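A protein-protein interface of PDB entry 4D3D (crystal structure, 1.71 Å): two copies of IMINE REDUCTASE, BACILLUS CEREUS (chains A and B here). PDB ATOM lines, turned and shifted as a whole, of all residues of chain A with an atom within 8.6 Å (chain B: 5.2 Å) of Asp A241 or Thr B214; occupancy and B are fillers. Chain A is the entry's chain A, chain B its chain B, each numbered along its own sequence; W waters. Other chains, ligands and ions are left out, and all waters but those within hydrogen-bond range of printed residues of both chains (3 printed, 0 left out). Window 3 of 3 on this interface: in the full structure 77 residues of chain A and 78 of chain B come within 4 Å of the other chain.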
ATOM      1  N   LEU A 185      -9.477 -23.777 -13.883  1.00  0.00           N
ATOM      2  CA  LEU A 185     -10.264 -22.537 -13.446  1.00  0.00           C
ATOM      3  C   LEU A 185     -10.817 -21.750 -14.613  1.00  0.00           C
ATOM      4  O   LEU A 185     -12.045 -21.529 -14.719  1.00  0.00           O
ATOM      5  CB  LEU A 185      -9.420 -21.648 -12.493  1.00  0.00           C
ATOM      6  CG  LEU A 185     -10.069 -20.369 -11.934  1.00  0.00           C
ATOM      7  CD1 LEU A 185     -10.267 -19.339 -13.016  1.00  0.00           C
ATOM      8  CD2 LEU A 185     -11.345 -20.677 -11.187  1.00  0.00           C
ATOM      9  N   TYR A 186      -9.976 -21.336 -15.546  1.00  0.00           N
ATOM     10  CA  TYR A 186     -10.422 -20.632 -16.694  1.00  0.00           C
ATOM     11  C   TYR A 186     -11.423 -21.437 -17.554  1.00  0.00           C
ATOM     12  O   TYR A 186     -12.424 -20.920 -18.088  1.00  0.00           O
ATOM     13  CB  TYR A 186      -9.224 -20.221 -17.575  1.00  0.00           C
ATOM     14  CG  TYR A 186      -8.460 -19.019 -16.980  1.00  0.00           C
ATOM     15  CD1 TYR A 186      -7.468 -19.184 -16.039  1.00  0.00           C
ATOM     16  CD2 TYR A 186      -8.777 -17.730 -17.368  1.00  0.00           C
ATOM     17  CE1 TYR A 186      -6.760 -18.071 -15.524  1.00  0.00           C
ATOM     18  CE2 TYR A 186      -8.128 -16.612 -16.790  1.00  0.00           C
ATOM     19  CZ  TYR A 186      -7.084 -16.822 -15.930  1.00  0.00           C
ATOM     20  OH  TYR A 186      -6.411 -15.682 -15.459  1.00  0.00           O
ATOM     21  N   ILE A 189     -14.976 -21.748 -15.475  1.00  0.00           N
ATOM     22  CA  ILE A 189     -15.795 -20.468 -15.327  1.00  0.00           C
ATOM     23  C   ILE A 189     -16.414 -20.068 -16.691  1.00  0.00           C
ATOM     24  O   ILE A 189     -17.518 -19.531 -16.745  1.00  0.00           O
ATOM     25  CB  ILE A 189     -14.991 -19.373 -14.604  1.00  0.00           C
ATOM     26  CG1 ILE A 189     -13.837 -18.888 -15.491  1.00  0.00           C
ATOM     27  CG2 ILE A 189     -14.591 -19.794 -13.220  1.00  0.00           C
ATOM     28  CD1 ILE A 189     -13.081 -17.729 -14.856  1.00  0.00           C
ATOM     29  N   PHE A 235     -18.235  -2.421 -18.967  1.00  0.00           N
ATOM     30  CA  PHE A 235     -18.693  -1.324 -18.037  1.00  0.00           C
ATOM     31  C   PHE A 235     -18.510  -1.649 -16.589  1.00  0.00           C
ATOM     32  O   PHE A 235     -17.922  -0.849 -15.813  1.00  0.00           O
ATOM     33  CB  PHE A 235     -20.161  -0.966 -18.261  1.00  0.00           C
ATOM     34  CG  PHE A 235     -20.643   0.158 -17.417  1.00  0.00           C
ATOM     35  CD1 PHE A 235     -20.395   1.482 -17.812  1.00  0.00           C
ATOM     36  CD2 PHE A 235     -21.253  -0.076 -16.207  1.00  0.00           C
ATOM     37  CE1 PHE A 235     -20.805   2.528 -17.006  1.00  0.00           C
ATOM     38  CE2 PHE A 235     -21.651   0.983 -15.377  1.00  0.00           C
ATOM     39  CZ  PHE A 235     -21.415   2.288 -15.796  1.00  0.00           C
ATOM     40  N   TYR A 236     -19.022  -2.804 -16.136  1.00  0.00           N
ATOM     41  CA  TYR A 236     -18.953  -3.126 -14.738  1.00  0.00           C
ATOM     42  C   TYR A 236     -17.602  -3.613 -14.196  1.00  0.00           C
ATOM     43  O   TYR A 236     -17.378  -3.600 -12.990  1.00  0.00           O
ATOM     44  CB  TYR A 236     -20.075  -4.111 -14.389  1.00  0.00           C
ATOM     45  CG  TYR A 236     -21.474  -3.494 -14.429  1.00  0.00           C
ATOM     46  CD1 TYR A 236     -21.875  -2.587 -13.471  1.00  0.00           C
ATOM     47  CD2 TYR A 236     -22.368  -3.845 -15.405  1.00  0.00           C
ATOM     48  CE1 TYR A 236     -23.127  -1.973 -13.540  1.00  0.00           C
ATOM     49  CE2 TYR A 236     -23.660  -3.279 -15.456  1.00  0.00           C
ATOM     50  CZ  TYR A 236     -24.029  -2.342 -14.506  1.00  0.00           C
ATOM     51  OH  TYR A 236     -25.330  -1.825 -14.532  1.00  0.00           O
ATOM     52  N   THR A 237     -16.722  -4.111 -15.079  1.00  0.00           N
ATOM     53  CA  THR A 237     -15.458  -4.748 -14.653  1.00  0.00           C
ATOM     54  C   THR A 237     -14.640  -3.919 -13.608  1.00  0.00           C
ATOM     55  O   THR A 237     -14.251  -4.468 -12.560  1.00  0.00           O
ATOM     56  CB  THR A 237     -14.639  -5.146 -15.925  1.00  0.00           C
ATOM     57  OG1 THR A 237     -15.223  -6.352 -16.468  1.00  0.00           O
ATOM     58  CG2 THR A 237     -13.162  -5.421 -15.650  1.00  0.00           C
ATOM     59  N   PRO A 238     -14.330  -2.653 -13.946  1.00  0.00           N
ATOM     60  CA  PRO A 238     -13.451  -1.872 -13.058  1.00  0.00           C
ATOM     61  C   PRO A 238     -14.167  -1.614 -11.718  1.00  0.00           C
ATOM     62  O   PRO A 238     -13.515  -1.614 -10.680  1.00  0.00           O
ATOM     63  CB  PRO A 238     -13.197  -0.593 -13.854  1.00  0.00           C
ATOM     64  CG  PRO A 238     -14.259  -0.508 -14.904  1.00  0.00           C
ATOM     65  CD  PRO A 238     -14.619  -1.954 -15.198  1.00  0.00           C
ATOM     66  N   ARG A 239     -15.500  -1.492 -11.741  1.00  0.00           N
ATOM     67  CA  ARG A 239     -16.262  -1.354 -10.481  1.00  0.00           C
ATOM     68  C   ARG A 239     -16.234  -2.567  -9.619  1.00  0.00           C
ATOM     69  O   ARG A 239     -16.014  -2.562  -8.383  1.00  0.00           O
ATOM     70  CB  ARG A 239     -17.712  -0.974 -10.806  1.00  0.00           C
ATOM     71  CG  ARG A 239     -17.829   0.367 -11.518  1.00  0.00           C
ATOM     72  CD  ARG A 239     -19.056   0.583 -12.367  1.00  0.00           C
ATOM     73  NE  ARG A 239     -20.258   0.256 -11.614  1.00  0.00           N
ATOM     74  CZ  ARG A 239     -21.291   1.098 -11.388  1.00  0.00           C
ATOM     75  NH1 ARG A 239     -21.320   2.333 -11.902  1.00  0.00           N
ATOM     76  NH2 ARG A 239     -22.316   0.637 -10.678  1.00  0.00           N
ATOM     77  N   LEU A 240     -16.463  -3.718 -10.260  1.00  0.00           N
ATOM     78  CA  LEU A 240     -16.366  -4.974  -9.563  1.00  0.00           C
ATOM     79  C   LEU A 240     -14.969  -5.193  -8.889  1.00  0.00           C
ATOM     80  O   LEU A 240     -14.900  -5.709  -7.766  1.00  0.00           O
ATOM     81  CB  LEU A 240     -16.646  -6.123 -10.570  1.00  0.00           C
ATOM     82  CG  LEU A 240     -18.170  -6.298 -10.870  1.00  0.00           C
ATOM     83  CD1 LEU A 240     -18.421  -6.977 -12.226  1.00  0.00           C
ATOM     84  CD2 LEU A 240     -18.811  -7.062  -9.734  1.00  0.00           C
ATOM     85  N   ASP A 241     -13.903  -4.800  -9.597  1.00  0.00           N
ATOM     86  CA  ASP A 241     -12.548  -5.003  -9.051  1.00  0.00           C
ATOM     87  C   ASP A 241     -12.258  -4.050  -7.873  1.00  0.00           C
ATOM     88  O   ASP A 241     -11.450  -4.382  -7.033  1.00  0.00           O
ATOM     89  CB  ASP A 241     -11.463  -4.840 -10.129  1.00  0.00           C
ATOM     90  CG  ASP A 241     -11.212  -6.133 -10.895  1.00  0.00           C
ATOM     91  OD1 ASP A 241     -11.652  -7.212 -10.382  1.00  0.00           O
ATOM     92  OD2 ASP A 241     -10.599  -6.034 -11.988  1.00  0.00           O
ATOM     93  N   GLU A 242     -12.965  -2.933  -7.811  1.00  0.00           N
ATOM     94  CA  GLU A 242     -12.936  -2.039  -6.605  1.00  0.00           C
ATOM     95  C   GLU A 242     -13.938  -2.439  -5.508  1.00  0.00           C
ATOM     96  O   GLU A 242     -13.865  -1.948  -4.409  1.00  0.00           O
ATOM     97  CB  GLU A 242     -13.163  -0.614  -7.051  1.00  0.00           C
ATOM     98  CG  GLU A 242     -11.948  -0.047  -7.778  1.00  0.00           C
ATOM     99  N   GLY A 243     -14.797  -3.428  -5.751  1.00  0.00           N
ATOM    100  CA  GLY A 243     -15.770  -3.873  -4.768  1.00  0.00           C
ATOM    101  C   GLY A 243     -16.900  -2.866  -4.600  1.00  0.00           C
ATOM    102  O   GLY A 243     -17.571  -2.837  -3.557  1.00  0.00           O
ATOM    103  N   GLU A 244     -17.138  -2.068  -5.624  1.00  0.00           N
ATOM    104  CA  GLU A 244     -18.089  -0.940  -5.615  1.00  0.00           C
ATOM    105  C   GLU A 244     -19.348  -1.244  -6.398  1.00  0.00           C
ATOM    106  O   GLU A 244     -19.255  -1.574  -7.578  1.00  0.00           O
ATOM    107  CB  GLU A 244     -17.432   0.321  -6.218  1.00  0.00           C
ATOM    108  CG  GLU A 244     -16.350   0.911  -5.288  1.00  0.00           C
ATOM    109  CD  GLU A 244     -16.897   1.272  -3.896  1.00  0.00           C
ATOM    110  OE1 GLU A 244     -17.883   2.034  -3.839  1.00  0.00           O
ATOM    111  OE2 GLU A 244     -16.379   0.800  -2.853  1.00  0.00           O
ATOM    112  N   HIS A 245     -20.503  -1.063  -5.741  1.00  0.00           N
ATOM    113  CA  HIS A 245     -21.843  -1.356  -6.363  1.00  0.00           C
ATOM    114  C   HIS A 245     -22.810  -0.144  -6.293  1.00  0.00           C
ATOM    115  O   HIS A 245     -23.969  -0.294  -5.942  1.00  0.00           O
ATOM    116  CB  HIS A 245     -22.474  -2.558  -5.675  1.00  0.00           C
ATOM    117  CG  HIS A 245     -21.575  -3.752  -5.638  1.00  0.00           C
ATOM    118  ND1 HIS A 245     -21.148  -4.398  -6.790  1.00  0.00           N
ATOM    119  CD2 HIS A 245     -20.972  -4.379  -4.604  1.00  0.00           C
ATOM    120  CE1 HIS A 245     -20.374  -5.401  -6.456  1.00  0.00           C
ATOM    121  NE2 HIS A 245     -20.223  -5.404  -5.140  1.00  0.00           N
ATOM    122  N   THR A 297     -25.076  -5.522  -9.639  1.00  0.00           N
ATOM    123  CA  THR A 297     -23.784  -6.206  -9.455  1.00  0.00           C
ATOM    124  C   THR A 297     -23.513  -6.585  -8.007  1.00  0.00           C
ATOM    125  O   THR A 297     -22.679  -7.481  -7.731  1.00  0.00           O
ATOM    126  CB  THR A 297     -22.551  -5.416 -10.005  1.00  0.00           C
ATOM    127  OG1 THR A 297     -22.419  -4.139  -9.290  1.00  0.00           O
ATOM    128  CG2 THR A 297     -22.633  -5.206 -11.407  1.00  0.00           C
ATOM    129  N   ILE A 300     -23.238 -10.241  -6.600  1.00  0.00           N
ATOM    130  CA  ILE A 300     -22.002 -11.069  -6.445  1.00  0.00           C
ATOM    131  C   ILE A 300     -21.731 -11.373  -4.986  1.00  0.00           C
ATOM    132  O   ILE A 300     -21.169 -12.407  -4.632  1.00  0.00           O
ATOM    133  CB  ILE A 300     -20.837 -10.450  -7.199  1.00  0.00           C
ATOM    134  CG1 ILE A 300     -19.752 -11.531  -7.448  1.00  0.00           C
ATOM    135  CG2 ILE A 300     -20.240  -9.330  -6.429  1.00  0.00           C
ATOM    136  CD1 ILE A 300     -18.587 -11.106  -8.338  1.00  0.00           C
ATOM    137  N   LYS A 304     -20.826 -14.947  -3.265  1.00  0.00           N
ATOM    138  CA  LYS A 304     -19.596 -15.092  -2.351  1.00  0.00           C
ATOM    139  C   LYS A 304     -19.841 -15.581  -0.892  1.00  0.00           C
ATOM    140  O   LYS A 304     -21.001 -15.646  -0.470  1.00  0.00           O
ATOM    141  CB  LYS A 304     -18.855 -13.795  -2.334  1.00  0.00           C
ATOM    142  CG  LYS A 304     -18.191 -13.449  -3.616  1.00  0.00           C
ATOM    143  CD  LYS A 304     -17.483 -12.097  -3.585  1.00  0.00           C
ATOM    144  CE  LYS A 304     -16.510 -12.096  -4.733  1.00  0.00           C
ATOM    145  NZ  LYS A 304     -15.507 -11.028  -4.741  1.00  0.00           N
ATOM    146  N   LEU B 205     -17.484 -15.036 -12.117  1.00  0.00           N
ATOM    147  CA  LEU B 205     -16.533 -14.083 -11.525  1.00  0.00           C
ATOM    148  C   LEU B 205     -16.293 -14.382 -10.044  1.00  0.00           C
ATOM    149  O   LEU B 205     -15.119 -14.330  -9.554  1.00  0.00           O
ATOM    150  CB  LEU B 205     -16.973 -12.655 -11.761  1.00  0.00           C
ATOM    151  CG  LEU B 205     -16.082 -11.582 -11.154  1.00  0.00           C
ATOM    152  CD1 LEU B 205     -14.670 -11.664 -11.755  1.00  0.00           C
ATOM    153  CD2 LEU B 205     -16.731 -10.259 -11.431  1.00  0.00           C
ATOM    154  N   ASN B 209     -12.630 -15.001  -8.557  1.00  0.00           N
ATOM    155  CA  ASN B 209     -12.135 -14.269  -7.350  1.00  0.00           C
ATOM    156  C   ASN B 209     -11.669 -15.213  -6.245  1.00  0.00           C
ATOM    157  O   ASN B 209     -10.621 -14.954  -5.626  1.00  0.00           O
ATOM    158  CB  ASN B 209     -13.185 -13.266  -6.766  1.00  0.00           C
ATOM    159  CG  ASN B 209     -13.569 -12.091  -7.660  1.00  0.00           C
ATOM    160  OD1 ASN B 209     -14.593 -11.426  -7.349  1.00  0.00           O
ATOM    161  ND2 ASN B 209     -12.863 -11.794  -8.708  1.00  0.00           N
ATOM    162  N   GLY B 212      -8.164 -16.264  -6.873  1.00  0.00           N
ATOM    163  CA  GLY B 212      -7.196 -15.212  -7.052  1.00  0.00           C
ATOM    164  C   GLY B 212      -7.226 -14.408  -8.321  1.00  0.00           C
ATOM    165  O   GLY B 212      -6.346 -13.590  -8.570  1.00  0.00           O
ATOM    166  N   ILE B 213      -8.265 -14.573  -9.141  1.00  0.00           N
ATOM    167  CA  ILE B 213      -8.296 -13.913 -10.427  1.00  0.00           C
ATOM    168  C   ILE B 213      -9.272 -12.752 -10.393  1.00  0.00           C
ATOM    169  O   ILE B 213     -10.407 -12.895  -9.912  1.00  0.00           O
ATOM    170  CB  ILE B 213      -8.772 -14.930 -11.518  1.00  0.00           C
ATOM    171  CG1 ILE B 213      -7.860 -16.158 -11.645  1.00  0.00           C
ATOM    172  CG2 ILE B 213      -8.927 -14.248 -12.841  1.00  0.00           C
ATOM    173  CD1 ILE B 213      -6.402 -15.781 -11.835  1.00  0.00           C
ATOM    174  N   THR B 214      -8.900 -11.643 -10.998  1.00  0.00           N
ATOM    175  CA  THR B 214      -9.693 -10.417 -11.015  1.00  0.00           C
ATOM    176  C   THR B 214     -10.692 -10.340 -12.195  1.00  0.00           C
ATOM    177  O   THR B 214     -10.617 -11.119 -13.175  1.00  0.00           O
ATOM    178  CB  THR B 214      -8.828  -9.158 -11.092  1.00  0.00           C
ATOM    179  OG1 THR B 214      -8.132  -9.094 -12.337  1.00  0.00           O
ATOM    180  CG2 THR B 214      -7.832  -9.210  -9.946  1.00  0.00           C
ATOM    181  N   ALA B 215     -11.620  -9.385 -12.114  1.00  0.00           N
ATOM    182  CA  ALA B 215     -12.485  -9.165 -13.236  1.00  0.00           C
ATOM    183  C   ALA B 215     -11.724  -8.679 -14.459  1.00  0.00           C
ATOM    184  O   ALA B 215     -12.044  -9.035 -15.569  1.00  0.00           O
ATOM    185  CB  ALA B 215     -13.599  -8.221 -12.892  1.00  0.00           C
ATOM    186  N   GLU B 216     -10.656  -7.898 -14.243  1.00  0.00           N
ATOM    187  CA  GLU B 216      -9.831  -7.452 -15.388  1.00  0.00           C
ATOM    188  C   GLU B 216      -9.159  -8.617 -16.128  1.00  0.00           C
ATOM    189  O   GLU B 216      -9.170  -8.655 -17.386  1.00  0.00           O
ATOM    190  CB  GLU B 216      -8.766  -6.433 -14.867  1.00  0.00           C
ATOM    191  CG  GLU B 216      -7.916  -5.851 -16.007  1.00  0.00           C
ATOM    192  CD  GLU B 216      -8.704  -4.924 -16.927  1.00  0.00           C
ATOM    193  OE1 GLU B 216      -9.818  -4.453 -16.535  1.00  0.00           O
ATOM    194  OE2 GLU B 216      -8.212  -4.658 -18.045  1.00  0.00           O
ATOM    195  N   GLN B 217      -8.708  -9.581 -15.381  1.00  0.00           N
ATOM    196  CA  GLN B 217      -8.105 -10.827 -15.906  1.00  0.00           C
ATOM    197  C   GLN B 217      -9.150 -11.679 -16.662  1.00  0.00           C
ATOM    198  O   GLN B 217      -8.882 -12.174 -17.760  1.00  0.00           O
ATOM    199  CB  GLN B 217      -7.489 -11.643 -14.819  1.00  0.00           C
ATOM    200  CG  GLN B 217      -6.167 -11.069 -14.277  1.00  0.00           C
ATOM    201  CD  GLN B 217      -5.607 -11.921 -13.155  1.00  0.00           C
ATOM    202  OE1 GLN B 217      -6.162 -11.981 -12.077  1.00  0.00           O
ATOM    203  NE2 GLN B 217      -4.481 -12.576 -13.409  1.00  0.00           N
ATOM    204  N   PHE B 218     -10.351 -11.763 -16.088  1.00  0.00           N
ATOM    205  CA  PHE B 218     -11.436 -12.542 -16.711  1.00  0.00           C
ATOM    206  C   PHE B 218     -12.067 -11.901 -17.912  1.00  0.00           C
ATOM    207  O   PHE B 218     -12.571 -12.630 -18.807  1.00  0.00           O
ATOM    208  CB  PHE B 218     -12.489 -12.874 -15.600  1.00  0.00           C
ATOM    209  CG  PHE B 218     -13.584 -13.815 -16.022  1.00  0.00           C
ATOM    210  CD1 PHE B 218     -13.387 -14.868 -16.910  1.00  0.00           C
ATOM    211  CD2 PHE B 218     -14.849 -13.716 -15.382  1.00  0.00           C
ATOM    212  CE1 PHE B 218     -14.411 -15.744 -17.204  1.00  0.00           C
ATOM    213  CE2 PHE B 218     -15.867 -14.592 -15.671  1.00  0.00           C
ATOM    214  CZ  PHE B 218     -15.655 -15.596 -16.595  1.00  0.00           C
ATOM    215  N   LEU B 219     -12.089 -10.552 -17.979  1.00  0.00           N
ATOM    216  CA  LEU B 219     -12.713  -9.799 -19.023  1.00  0.00           C
ATOM    217  C   LEU B 219     -12.639 -10.351 -20.458  1.00  0.00           C
ATOM    218  O   LEU B 219     -13.659 -10.581 -21.102  1.00  0.00           O
ATOM    219  CB  LEU B 219     -12.213  -8.319 -19.006  1.00  0.00           C
ATOM    220  CG  LEU B 219     -12.671  -7.383 -20.073  1.00  0.00           C
ATOM    221  CD1 LEU B 219     -14.188  -7.215 -20.128  1.00  0.00           C
ATOM    222  CD2 LEU B 219     -11.980  -5.990 -19.962  1.00  0.00           C
HETATM  223  O   HOH W   1     -13.264  -8.738  -9.126  1.00  0.00           O
HETATM  224  O   HOH W   2     -14.708  -9.117 -16.298  1.00  0.00           O
HETATM  225  O   HOH W   3     -15.645  -9.046  -8.277  1.00  0.00           O
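No position is printed for both chains.
Of the 11 pairs that touch across the chains among the printed residues, none has its exchanged pair printed and touching as well.
Water W1 lies within hydrogen-bond range of the side-chain carboxylate of Asp A241 (2.6 Å), the side-chain amide nitrogen of Asn B209 (3.1 Å) and the backbone NH of Ala B215 (3.5 Å).
Water W3 bridges OD1 of Asn B209 (2.8 Å) and O of Leu A240 (3.5 Å).
Water W2 lies within hydrogen-bond range of the backbone carbonyl oxygen (O) of Ala B215 (2.8 Å), the side-chain hydroxyl (OG1) of Thr A237 (2.8 Å) and the backbone NH (N) of Leu B219 (3.4 Å).
O of Leu B205 lies close to ND2 of Asn B209, 3.5 Å away.
The side-chain amide nitrogen (ND2) of Asn B209 is in hydrogen-bond range of the backbone carbonyl oxygen (O) of Ile B213 (2.9 Å).
N of Glu B216 lies close to OG1 of Thr B214 (3.4 Å).
N of Thr B214 is in hydrogen-bond range of OE1 of Gln B217 (3.0 Å).
Among the printed residues, pairs that only touch across the chains: Ile A189 with Phe B218 (3.3 Å), Asp A241 with Thr B214 (3.5 Å), Thr A237 with Glu B216 (3.6 Å), Tyr A186 with Ile B213 (3.6 Å), Ile A300 with Leu B205 (3.7 Å), Thr A237 with Ala B215 (3.8 Å), Leu A240 with Leu B205 (3.8 Å) and Thr A237 with Leu B219 (3.9 Å).
Printed residues of chain B that touch a printed residue of chain A: Leu B205, Asn B209, Ile B213, Thr B214, Ala B215, Glu B216, Phe B218 and Leu B219.
Hydrophobic or aromatic side chains of chain B within 4 Å of the printed part of chain A: Leu B205, Ile B213, Ala B215, Phe B218 and Leu B219.
Among the printed residues, no Asp or Glu carboxylate lies within 4 Å of a Lys or Arg side-chain nitrogen of the other chain.
N of Ala B215 lies within hydrogen-bond range of OD1 of Asp A241 (2.8 Å).
The side-chain carboxylate (OD2) of Asp A241 lies within hydrogen-bond range of the backbone NH (N) of Glu B216 (2.9 Å).
The side-chain amide oxygen of Asn B209 sits at hydrogen-bond distance from the side-chain amino group of Lys A304 (2.8 Å).
Of chain B, only Thr B214, Ala B215 and Glu B216 come within 4 Å of Asp A241.
Thr B214 touches one residue of chain A.
Of chain A, only Thr A237 (3.8 Å) and Asp A241 (2.8 Å) come within 4 Å of Ala B215.
Of the printed residues of chain A, Asn B209 touches Lys A304.
Printed residues of chain B within 4 Å of Ile A189: Phe B218 (3.3 Å).
Printed residues of chain B within 4 Å of Leu A240: Leu B205 (3.8 Å).
Of the printed residues of chain A, Leu B205 touches Leu A240 (3.8 Å) and Ile A300 (3.7 Å).
Tyr A236 touches none of the printed residues of chain B.
The nearest residue of chain B that does not touch Asp A241 is Asn B209 (5.0 Å).
The nearest printed residue of chain A that does not touch Thr B214 is Thr A237 (6.5 Å).
The nearest printed residue of chain B that does not touch Thr A237 is Gln B217 (6.1 Å).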
